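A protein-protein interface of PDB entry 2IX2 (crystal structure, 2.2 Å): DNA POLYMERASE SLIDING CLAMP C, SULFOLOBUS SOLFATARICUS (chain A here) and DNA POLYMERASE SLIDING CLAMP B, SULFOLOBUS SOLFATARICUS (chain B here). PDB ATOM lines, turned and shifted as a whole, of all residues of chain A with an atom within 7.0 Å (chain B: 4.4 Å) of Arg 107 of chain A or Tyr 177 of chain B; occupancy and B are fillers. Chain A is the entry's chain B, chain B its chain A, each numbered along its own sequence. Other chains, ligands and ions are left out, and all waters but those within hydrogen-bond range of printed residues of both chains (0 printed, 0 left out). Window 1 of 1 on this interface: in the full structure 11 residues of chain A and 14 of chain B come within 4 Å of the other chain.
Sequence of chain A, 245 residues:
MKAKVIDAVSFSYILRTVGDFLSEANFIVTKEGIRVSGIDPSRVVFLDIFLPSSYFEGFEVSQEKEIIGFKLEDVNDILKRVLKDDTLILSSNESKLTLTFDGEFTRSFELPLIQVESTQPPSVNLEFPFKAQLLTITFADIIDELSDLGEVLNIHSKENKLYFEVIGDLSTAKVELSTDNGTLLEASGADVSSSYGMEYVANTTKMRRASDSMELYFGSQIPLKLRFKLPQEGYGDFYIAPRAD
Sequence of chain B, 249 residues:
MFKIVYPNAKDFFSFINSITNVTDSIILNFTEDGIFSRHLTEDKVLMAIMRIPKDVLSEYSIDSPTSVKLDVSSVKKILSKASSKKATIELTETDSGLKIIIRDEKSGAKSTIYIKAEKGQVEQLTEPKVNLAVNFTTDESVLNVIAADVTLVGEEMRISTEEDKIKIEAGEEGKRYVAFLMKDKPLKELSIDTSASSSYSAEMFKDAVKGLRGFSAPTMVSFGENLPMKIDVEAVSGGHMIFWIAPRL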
ATOM      1  N   ILE A  78      25.057 -26.307  17.275  1.00  0.00           N
ATOM      2  CA  ILE A  78      23.838 -25.916  16.559  1.00  0.00           C
ATOM      3  C   ILE A  78      23.740 -26.685  15.242  1.00  0.00           C
ATOM      4  O   ILE A  78      22.662 -27.134  14.869  1.00  0.00           O
ATOM      5  CB  ILE A  78      23.772 -24.383  16.314  1.00  0.00           C
ATOM      6  CG1 ILE A  78      23.525 -23.639  17.633  1.00  0.00           C
ATOM      7  CG2 ILE A  78      22.667 -24.035  15.304  1.00  0.00           C
ATOM      8  CD1 ILE A  78      23.935 -22.168  17.609  1.00  0.00           C
ATOM      9  N   ARG A  81      22.284 -30.137  14.767  1.00  0.00           N
ATOM     10  CA  ARG A  81      20.814 -30.154  14.763  1.00  0.00           C
ATOM     11  C   ARG A  81      20.212 -30.138  13.357  1.00  0.00           C
ATOM     12  O   ARG A  81      19.006 -30.315  13.192  1.00  0.00           O
ATOM     13  CB  ARG A  81      20.262 -28.972  15.565  1.00  0.00           C
ATOM     14  CG  ARG A  81      20.642 -28.946  17.037  1.00  0.00           C
ATOM     15  CD  ARG A  81      19.734 -29.810  17.888  1.00  0.00           C
ATOM     16  NE  ARG A  81      20.026 -31.226  17.706  1.00  0.00           N
ATOM     17  CZ  ARG A  81      19.162 -32.135  17.263  1.00  0.00           C
ATOM     18  NH1 ARG A  81      17.915 -31.793  16.949  1.00  0.00           N
ATOM     19  NH2 ARG A  81      19.559 -33.397  17.142  1.00  0.00           N
ATOM     20  N   VAL A  82      21.060 -29.903  12.355  1.00  0.00           N
ATOM     21  CA  VAL A  82      20.657 -29.933  10.950  1.00  0.00           C
ATOM     22  C   VAL A  82      19.938 -31.239  10.599  1.00  0.00           C
ATOM     23  O   VAL A  82      20.295 -32.316  11.097  1.00  0.00           O
ATOM     24  CB  VAL A  82      21.861 -29.698   9.991  1.00  0.00           C
ATOM     25  CG1 VAL A  82      22.835 -30.891  10.002  1.00  0.00           C
ATOM     26  CG2 VAL A  82      21.370 -29.409   8.579  1.00  0.00           C
ATOM     27  N   LEU A  83      18.901 -31.126   9.775  1.00  0.00           N
ATOM     28  CA  LEU A  83      18.241 -32.296   9.210  1.00  0.00           C
ATOM     29  C   LEU A  83      18.675 -32.525   7.755  1.00  0.00           C
ATOM     30  O   LEU A  83      19.257 -31.643   7.115  1.00  0.00           O
ATOM     31  CB  LEU A  83      16.724 -32.170   9.331  1.00  0.00           C
ATOM     32  CG  LEU A  83      16.144 -32.240  10.752  1.00  0.00           C
ATOM     33  CD1 LEU A  83      14.670 -31.817  10.741  1.00  0.00           C
ATOM     34  CD2 LEU A  83      16.314 -33.641  11.393  1.00  0.00           C
ATOM     35  N   LYS A  84      18.418 -33.729   7.257  1.00  0.00           N
ATOM     36  CA  LYS A  84      18.620 -34.044   5.856  1.00  0.00           C
ATOM     37  C   LYS A  84      17.656 -33.164   5.055  1.00  0.00           C
ATOM     38  O   LYS A  84      16.467 -33.092   5.379  1.00  0.00           O
ATOM     39  CB  LYS A  84      18.319 -35.529   5.611  1.00  0.00           C
ATOM     40  CG  LYS A  84      18.792 -36.069   4.255  1.00  0.00           C
ATOM     41  CD  LYS A  84      17.983 -37.363   3.906  1.00  0.00           C
ATOM     42  CE  LYS A  84      18.358 -37.605   2.220  1.00  0.00           C
ATOM     43  NZ  LYS A  84      17.686 -39.295   2.215  1.00  0.00           N
ATOM     44  N   ASP A  86      17.711 -29.890   4.881  1.00  0.00           N
ATOM     45  CA  ASP A  86      17.721 -28.532   5.419  1.00  0.00           C
ATOM     46  C   ASP A  86      18.502 -27.557   4.537  1.00  0.00           C
ATOM     47  O   ASP A  86      19.601 -27.861   4.051  1.00  0.00           O
ATOM     48  CB  ASP A  86      18.303 -28.492   6.839  1.00  0.00           C
ATOM     49  CG  ASP A  86      17.251 -28.690   7.936  1.00  0.00           C
ATOM     50  OD1 ASP A  86      17.681 -28.782   9.107  1.00  0.00           O
ATOM     51  OD2 ASP A  86      16.020 -28.741   7.659  1.00  0.00           O
ATOM     52  N   LEU A  88      20.121 -23.614   4.937  1.00  0.00           N
ATOM     53  CA  LEU A  88      20.647 -22.823   6.058  1.00  0.00           C
ATOM     54  C   LEU A  88      20.874 -21.361   5.681  1.00  0.00           C
ATOM     55  O   LEU A  88      21.537 -21.066   4.690  1.00  0.00           O
ATOM     56  CB  LEU A  88      21.943 -23.434   6.611  1.00  0.00           C
ATOM     57  CG  LEU A  88      22.733 -22.671   7.692  1.00  0.00           C
ATOM     58  CD1 LEU A  88      22.013 -22.654   9.046  1.00  0.00           C
ATOM     59  CD2 LEU A  88      24.120 -23.260   7.844  1.00  0.00           C
ATOM     60  N   LEU A  99      21.535 -18.702  13.058  1.00  0.00           N
ATOM     61  CA  LEU A  99      21.523 -19.850  12.150  1.00  0.00           C
ATOM     62  C   LEU A  99      20.097 -20.394  11.995  1.00  0.00           C
ATOM     63  O   LEU A  99      19.494 -20.902  12.953  1.00  0.00           O
ATOM     64  CB  LEU A  99      22.485 -20.938  12.638  1.00  0.00           C
ATOM     65  CG  LEU A  99      23.933 -20.495  12.866  1.00  0.00           C
ATOM     66  CD1 LEU A  99      24.672 -21.442  13.792  1.00  0.00           C
ATOM     67  CD2 LEU A  99      24.664 -20.357  11.532  1.00  0.00           C
ATOM     68  N   THR A 100      19.570 -20.263  10.782  1.00  0.00           N
ATOM     69  CA  THR A 100      18.197 -20.653  10.464  1.00  0.00           C
ATOM     70  C   THR A 100      18.156 -21.883   9.552  1.00  0.00           C
ATOM     71  O   THR A 100      18.714 -21.864   8.450  1.00  0.00           O
ATOM     72  CB  THR A 100      17.444 -19.486   9.791  1.00  0.00           C
ATOM     73  OG1 THR A 100      17.346 -18.387  10.709  1.00  0.00           O
ATOM     74  CG2 THR A 100      16.041 -19.912   9.367  1.00  0.00           C
ATOM     75  N   PHE A 101      17.495 -22.944  10.017  1.00  0.00           N
ATOM     76  CA  PHE A 101      17.297 -24.149   9.202  1.00  0.00           C
ATOM     77  C   PHE A 101      15.920 -24.136   8.541  1.00  0.00           C
ATOM     78  O   PHE A 101      14.937 -23.744   9.170  1.00  0.00           O
ATOM     79  CB  PHE A 101      17.476 -25.426  10.036  1.00  0.00           C
ATOM     80  CG  PHE A 101      18.869 -25.607  10.587  1.00  0.00           C
ATOM     81  CD1 PHE A 101      19.114 -25.463  11.950  1.00  0.00           C
ATOM     82  CD2 PHE A 101      19.930 -25.916   9.749  1.00  0.00           C
ATOM     83  CE1 PHE A 101      20.409 -25.621  12.475  1.00  0.00           C
ATOM     84  CE2 PHE A 101      21.228 -26.081  10.260  1.00  0.00           C
ATOM     85  CZ  PHE A 101      21.460 -25.935  11.632  1.00  0.00           C
ATOM     86  N   ASP A 102      15.861 -24.563   7.278  1.00  0.00           N
ATOM     87  CA  ASP A 102      14.593 -24.641   6.521  1.00  0.00           C
ATOM     88  C   ASP A 102      14.427 -26.010   5.871  1.00  0.00           C
ATOM     89  O   ASP A 102      15.338 -26.495   5.209  1.00  0.00           O
ATOM     90  CB  ASP A 102      14.548 -23.567   5.434  1.00  0.00           C
ATOM     91  CG  ASP A 102      13.745 -22.338   5.846  1.00  0.00           C
ATOM     92  OD1 ASP A 102      12.476 -22.381   5.775  1.00  0.00           O
ATOM     93  OD2 ASP A 102      14.387 -21.315   6.201  1.00  0.00           O
ATOM     94  N   GLY A 103      13.265 -26.629   6.044  1.00  0.00           N
ATOM     95  CA  GLY A 103      13.016 -27.948   5.457  1.00  0.00           C
ATOM     96  C   GLY A 103      11.688 -28.538   5.884  1.00  0.00           C
ATOM     97  O   GLY A 103      10.643 -28.098   5.423  1.00  0.00           O
ATOM     98  N   GLU A 104      11.736 -29.544   6.760  1.00  0.00           N
ATOM     99  CA  GLU A 104      10.538 -30.089   7.397  1.00  0.00           C
ATOM    100  C   GLU A 104       9.742 -28.941   8.012  1.00  0.00           C
ATOM    101  O   GLU A 104       8.524 -28.855   7.829  1.00  0.00           O
ATOM    102  CB  GLU A 104      10.891 -31.117   8.479  1.00  0.00           C
ATOM    103  CG  GLU A 104      11.695 -32.340   7.995  1.00  0.00           C
ATOM    104  CD  GLU A 104      11.475 -33.591   8.893  1.00  0.00           C
ATOM    105  OE1 GLU A 104      10.286 -34.113   8.919  1.00  0.00           O
ATOM    106  OE2 GLU A 104      12.497 -34.053   9.571  1.00  0.00           O
ATOM    107  N   PHE A 105      10.444 -28.071   8.739  1.00  0.00           N
ATOM    108  CA  PHE A 105       9.882 -26.825   9.260  1.00  0.00           C
ATOM    109  C   PHE A 105      10.992 -25.812   9.537  1.00  0.00           C
ATOM    110  O   PHE A 105      12.171 -26.130   9.396  1.00  0.00           O
ATOM    111  CB  PHE A 105       9.002 -27.075  10.499  1.00  0.00           C
ATOM    112  CG  PHE A 105       9.738 -27.645  11.685  1.00  0.00           C
ATOM    113  CD1 PHE A 105       9.907 -26.873  12.841  1.00  0.00           C
ATOM    114  CD2 PHE A 105      10.242 -28.960  11.659  1.00  0.00           C
ATOM    115  CE1 PHE A 105      10.570 -27.393  13.950  1.00  0.00           C
ATOM    116  CE2 PHE A 105      10.920 -29.486  12.760  1.00  0.00           C
ATOM    117  CZ  PHE A 105      11.081 -28.700  13.908  1.00  0.00           C
ATOM    118  N   THR A 106      10.617 -24.588   9.902  1.00  0.00           N
ATOM    119  CA  THR A 106      11.609 -23.541  10.175  1.00  0.00           C
ATOM    120  C   THR A 106      11.990 -23.505  11.649  1.00  0.00           C
ATOM    121  O   THR A 106      11.130 -23.583  12.529  1.00  0.00           O
ATOM    122  CB  THR A 106      11.109 -22.137   9.758  1.00  0.00           C
ATOM    123  OG1 THR A 106      10.550 -22.195   8.438  1.00  0.00           O
ATOM    124  CG2 THR A 106      12.263 -21.132   9.767  1.00  0.00           C
ATOM    125  N   ARG A 107      13.285 -23.377  11.908  1.00  0.00           N
ATOM    126  CA  ARG A 107      13.788 -23.273  13.273  1.00  0.00           C
ATOM    127  C   ARG A 107      15.081 -22.494  13.294  1.00  0.00           C
ATOM    128  O   ARG A 107      15.923 -22.657  12.421  1.00  0.00           O
ATOM    129  CB  ARG A 107      13.959 -24.655  13.898  1.00  0.00           C
ATOM    130  CG  ARG A 107      14.751 -25.588  13.045  1.00  0.00           C
ATOM    131  CD  ARG A 107      14.214 -26.996  13.101  1.00  0.00           C
ATOM    132  NE  ARG A 107      15.040 -27.828  12.243  1.00  0.00           N
ATOM    133  CZ  ARG A 107      16.181 -28.383  12.626  1.00  0.00           C
ATOM    134  NH1 ARG A 107      16.614 -28.227  13.873  1.00  0.00           N
ATOM    135  NH2 ARG A 107      16.879 -29.103  11.759  1.00  0.00           N
ATOM    136  N   SER A 108      15.236 -21.639  14.294  1.00  0.00           N
ATOM    137  CA  SER A 108      16.377 -20.740  14.334  1.00  0.00           C
ATOM    138  C   SER A 108      17.125 -20.755  15.651  1.00  0.00           C
ATOM    139  O   SER A 108      16.516 -20.833  16.724  1.00  0.00           O
ATOM    140  CB  SER A 108      15.931 -19.323  14.010  1.00  0.00           C
ATOM    141  OG  SER A 108      15.738 -19.201  12.618  1.00  0.00           O
ATOM    142  N   PHE A 109      18.446 -20.645  15.544  1.00  0.00           N
ATOM    143  CA  PHE A 109      19.348 -20.623  16.691  1.00  0.00           C
ATOM    144  C   PHE A 109      20.189 -19.348  16.701  1.00  0.00           C
ATOM    145  O   PHE A 109      20.843 -18.996  15.700  1.00  0.00           O
ATOM    146  CB  PHE A 109      20.263 -21.854  16.689  1.00  0.00           C
ATOM    147  CG  PHE A 109      19.532 -23.160  16.828  1.00  0.00           C
ATOM    148  CD1 PHE A 109      19.391 -23.761  18.075  1.00  0.00           C
ATOM    149  CD2 PHE A 109      19.005 -23.806  15.703  1.00  0.00           C
ATOM    150  CE1 PHE A 109      18.722 -24.980  18.209  1.00  0.00           C
ATOM    151  CE2 PHE A 109      18.340 -25.022  15.819  1.00  0.00           C
ATOM    152  CZ  PHE A 109      18.195 -25.615  17.076  1.00  0.00           C
ATOM    153  N   GLU A 110      20.170 -18.679  17.851  1.00  0.00           N
ATOM    154  CA  GLU A 110      20.838 -17.403  18.049  1.00  0.00           C
ATOM    155  C   GLU A 110      22.133 -17.608  18.821  1.00  0.00           C
ATOM    156  O   GLU A 110      22.155 -18.283  19.868  1.00  0.00           O
ATOM    157  CB  GLU A 110      19.919 -16.467  18.827  1.00  0.00           C
ATOM    158  CG  GLU A 110      19.921 -15.030  18.342  1.00  0.00           C
ATOM    159  CD  GLU A 110      18.873 -14.183  19.030  1.00  0.00           C
ATOM    160  OE1 GLU A 110      18.741 -14.293  20.271  1.00  0.00           O
ATOM    161  OE2 GLU A 110      18.190 -13.404  18.329  1.00  0.00           O
ATOM    162  N   VAL B 145      13.072 -33.958  17.181  1.00  0.00           N
ATOM    163  CA  VAL B 145      13.873 -32.828  16.714  1.00  0.00           C
ATOM    164  C   VAL B 145      13.688 -31.639  17.658  1.00  0.00           C
ATOM    165  O   VAL B 145      14.670 -31.040  18.097  1.00  0.00           O
ATOM    166  CB  VAL B 145      13.529 -32.418  15.261  1.00  0.00           C
ATOM    167  CG1 VAL B 145      14.285 -31.145  14.854  1.00  0.00           C
ATOM    168  CG2 VAL B 145      13.840 -33.555  14.288  1.00  0.00           C
ATOM    169  N   ASP B 149      16.428 -29.830  20.076  1.00  0.00           N
ATOM    170  CA  ASP B 149      16.689 -28.406  19.794  1.00  0.00           C
ATOM    171  C   ASP B 149      16.516 -27.543  21.049  1.00  0.00           C
ATOM    172  O   ASP B 149      17.355 -26.692  21.368  1.00  0.00           O
ATOM    173  CB  ASP B 149      15.728 -27.882  18.713  1.00  0.00           C
ATOM    174  CG  ASP B 149      15.961 -28.500  17.341  1.00  0.00           C
ATOM    175  OD1 ASP B 149      16.956 -29.215  17.149  1.00  0.00           O
ATOM    176  OD2 ASP B 149      15.135 -28.265  16.438  1.00  0.00           O
ATOM    177  N   VAL B 150      15.412 -27.770  21.753  1.00  0.00           N
ATOM    178  CA  VAL B 150      15.108 -27.041  22.986  1.00  0.00           C
ATOM    179  C   VAL B 150      16.149 -27.266  24.089  1.00  0.00           C
ATOM    180  O   VAL B 150      16.551 -26.318  24.755  1.00  0.00           O
ATOM    181  CB  VAL B 150      13.664 -27.365  23.488  1.00  0.00           C
ATOM    182  CG1 VAL B 150      13.433 -26.836  24.899  1.00  0.00           C
ATOM    183  CG2 VAL B 150      12.621 -26.802  22.508  1.00  0.00           C
ATOM    184  N   VAL B 153      19.530 -25.334  24.080  1.00  0.00           N
ATOM    185  CA  VAL B 153      19.514 -23.897  24.400  1.00  0.00           C
ATOM    186  C   VAL B 153      18.995 -23.489  25.798  1.00  0.00           C
ATOM    187  O   VAL B 153      19.319 -22.400  26.281  1.00  0.00           O
ATOM    188  CB  VAL B 153      18.747 -23.082  23.315  1.00  0.00           C
ATOM    189  CG1 VAL B 153      19.365 -23.296  21.923  1.00  0.00           C
ATOM    190  CG2 VAL B 153      17.279 -23.452  23.306  1.00  0.00           C
ATOM    191  N   ILE B 168       7.410 -22.309  18.937  1.00  0.00           N
ATOM    192  CA  ILE B 168       8.122 -22.905  20.055  1.00  0.00           C
ATOM    193  C   ILE B 168       9.363 -22.078  20.343  1.00  0.00           C
ATOM    194  O   ILE B 168      10.163 -21.820  19.440  1.00  0.00           O
ATOM    195  CB  ILE B 168       8.486 -24.376  19.781  1.00  0.00           C
ATOM    196  CG1 ILE B 168       7.208 -25.188  19.508  1.00  0.00           C
ATOM    197  CG2 ILE B 168       9.290 -24.962  20.959  1.00  0.00           C
ATOM    198  CD1 ILE B 168       7.443 -26.586  19.007  1.00  0.00           C
ATOM    199  N   GLU B 169       9.512 -21.662  21.601  1.00  0.00           N
ATOM    200  CA  GLU B 169      10.612 -20.788  22.020  1.00  0.00           C
ATOM    201  C   GLU B 169      11.388 -21.315  23.226  1.00  0.00           C
ATOM    202  O   GLU B 169      10.796 -21.671  24.243  1.00  0.00           O
ATOM    203  CB  GLU B 169      10.071 -19.402  22.368  1.00  0.00           C
ATOM    204  CG  GLU B 169       9.666 -18.561  21.179  1.00  0.00           C
ATOM    205  CD  GLU B 169       8.895 -17.312  21.596  1.00  0.00           C
ATOM    206  OE1 GLU B 169       7.761 -17.449  22.111  1.00  0.00           O
ATOM    207  OE2 GLU B 169       9.422 -16.197  21.402  1.00  0.00           O
ATOM    208  N   ALA B 170      12.715 -21.339  23.119  1.00  0.00           N
ATOM    209  CA  ALA B 170      13.564 -21.704  24.250  1.00  0.00           C
ATOM    210  C   ALA B 170      14.856 -20.891  24.289  1.00  0.00           C
ATOM    211  O   ALA B 170      15.277 -20.318  23.279  1.00  0.00           O
ATOM    212  CB  ALA B 170      13.856 -23.191  24.238  1.00  0.00           C
ATOM    213  N   ARG B 176      19.174 -18.279  22.094  1.00  0.00           N
ATOM    214  CA  ARG B 176      17.727 -18.412  21.883  1.00  0.00           C
ATOM    215  C   ARG B 176      17.329 -19.253  20.649  1.00  0.00           C
ATOM    216  O   ARG B 176      18.056 -19.303  19.645  1.00  0.00           O
ATOM    217  CB  ARG B 176      17.043 -17.036  21.872  1.00  0.00           C
ATOM    218  CG  ARG B 176      15.528 -17.108  21.799  1.00  0.00           C
ATOM    219  CD  ARG B 176      14.821 -15.966  22.535  1.00  0.00           C
ATOM    220  NE  ARG B 176      13.528 -16.428  23.058  1.00  0.00           N
ATOM    221  CZ  ARG B 176      13.315 -16.820  24.314  1.00  0.00           C
ATOM    222  NH1 ARG B 176      14.299 -16.784  25.207  1.00  0.00           N
ATOM    223  NH2 ARG B 176      12.109 -17.235  24.689  1.00  0.00           N
ATOM    224  N   TYR B 177      16.175 -19.915  20.756  1.00  0.00           N
ATOM    225  CA  TYR B 177      15.648 -20.789  19.715  1.00  0.00           C
ATOM    226  C   TYR B 177      14.177 -20.504  19.437  1.00  0.00           C
ATOM    227  O   TYR B 177      13.380 -20.347  20.368  1.00  0.00           O
ATOM    228  CB  TYR B 177      15.834 -22.257  20.121  1.00  0.00           C
ATOM    229  CG  TYR B 177      15.063 -23.295  19.304  1.00  0.00           C
ATOM    230  CD1 TYR B 177      13.914 -23.901  19.814  1.00  0.00           C
ATOM    231  CD2 TYR B 177      15.511 -23.695  18.047  1.00  0.00           C
ATOM    232  CE1 TYR B 177      13.226 -24.865  19.086  1.00  0.00           C
ATOM    233  CE2 TYR B 177      14.827 -24.657  17.305  1.00  0.00           C
ATOM    234  CZ  TYR B 177      13.690 -25.235  17.826  1.00  0.00           C
ATOM    235  OH  TYR B 177      13.029 -26.188  17.098  1.00  0.00           O
ATOM    236  N   VAL B 178      13.831 -20.423  18.151  1.00  0.00           N
ATOM    237  CA  VAL B 178      12.442 -20.306  17.716  1.00  0.00           C
ATOM    238  C   VAL B 178      12.136 -21.276  16.579  1.00  0.00           C
ATOM    239  O   VAL B 178      12.898 -21.376  15.609  1.00  0.00           O
ATOM    240  CB  VAL B 178      12.044 -18.860  17.300  1.00  0.00           C
ATOM    241  CG1 VAL B 178      11.959 -17.949  18.521  1.00  0.00           C
ATOM    242  CG2 VAL B 178      13.019 -18.290  16.280  1.00  0.00           C
ATOM    243  N   ALA B 179      11.027 -21.996  16.718  1.00  0.00           N
ATOM    244  CA  ALA B 179      10.545 -22.870  15.661  1.00  0.00           C
ATOM    245  C   ALA B 179       9.078 -22.596  15.332  1.00  0.00           C
ATOM    246  O   ALA B 179       8.291 -22.236  16.205  1.00  0.00           O
ATOM    247  CB  ALA B 179      10.732 -24.309  16.041  1.00  0.00           C
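Of chain B, only Val 145, Asp 149, Tyr 177, Val 178 and Ala 179 come within 4 Å of Arg 107 of chain A. Tyr 177 of chain B touches three residues of chain A. Of the printed residues of chain B, Phe 105 of chain A touches Ala 179. Of the printed residues of chain B, Ser 108 of chain A touches Arg 176 (3.6 Å), Tyr 177 (3.1 Å) and Val 178 (2.7 Å). Printed residues of chain A within 4 Å of Val 178 of chain B: Arg 107 (3.1 Å) and Ser 108 (2.7 Å). Of the printed residues of chain A, Ala 179 of chain B touches Phe 105, Thr 106 and Arg 107. Val 82 of chain A touches none of the printed residues of chain B. Asp 102 of chain A touches none of the printed residues of chain B. The nearest residue of chain A that does not touch Tyr 177 of chain B is Phe 105 of chain A (4.2 Å).
CG2 of Val 145 of chain B touches CD2 of Leu 83 of chain A (3.8 Å). CB of Ala 179 of chain B touches CE1 of Phe 105 of chain A, at 3.7 Å. Ala 179 of chain B touches Thr 106 of chain A (CA to O, 3.3 Å). Val 145 of chain B touches Arg 107 of chain A. CA of Arg 107 of chain A touches O of Val 178 of chain B (3.1 Å). Ser 108 of chain A touches Arg 176 of chain B. Ser 108 of chain A touches Tyr 177 of chain B. CZ of Phe 109 of chain A touches CG of Asp 149 of chain B, at 3.7 Å. CA of Phe 109 of chain A touches O of Arg 176 of chain B, at 3.5 Å. Tyr 177 of chain B touches Phe 109 of chain A.
OG of Ser 108 of chain A is in hydrogen-bond range of OG1 of Thr 100 of chain A, 2.6 Å away. The backbone NH (N) of Leu 83 of chain A sits at hydrogen-bond distance from the side-chain carboxylate (OD1) of Asp 86 of chain A (2.7 Å). The backbone NH (N) of Leu 99 of chain A sits at hydrogen-bond distance from the backbone carbonyl oxygen (O) of Phe 109 of chain A (2.7 Å). The backbone carbonyl oxygen of Ile 168 of chain B sits at hydrogen-bond distance from the backbone NH of Ala 179 of chain B. The backbone carbonyl oxygen (O) of Arg 81 of chain A is in hydrogen-bond range of the guanidinium group (NH2) of Arg 107 of chain A. The backbone NH (N) of Phe 101 of chain A lies within hydrogen-bond range of the backbone carbonyl oxygen (O) of Arg 107 of chain A.
Printed residues of chain A that touch a printed residue of chain B: Arg 81, Leu 83, Phe 105, Thr 106, Arg 107, Ser 108, Phe 109 and Glu 110. Hydrophobic or aromatic side chains of chain A that line the printed part of chain B: Leu 83, Phe 105 and Phe 109. Along chain A the printed residues that touch a printed residue of chain B span positions 81 to 110. Of the 11 printed residues of chain B, 7 touch a printed residue of chain A.
O of Val 178 of chain B is in hydrogen-bond range of N of Ser 108 of chain A, at 2.7 Å. The backbone carbonyl oxygen (O) of Arg 176 of chain B sits at hydrogen-bond distance from the backbone NH (N) of Glu 110 of chain A (2.8 Å). The side-chain carboxylate (OD1) of Asp 149 of chain B is in salt-bridge range of the guanidinium group (NH1) of Arg 81 of chain A (2.8 Å). The guanidinium group (NH1) of Arg 107 of chain A is in salt-bridge range of the side-chain carboxylate (OD2) of Asp 149 of chain B, 3.0 Å away.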
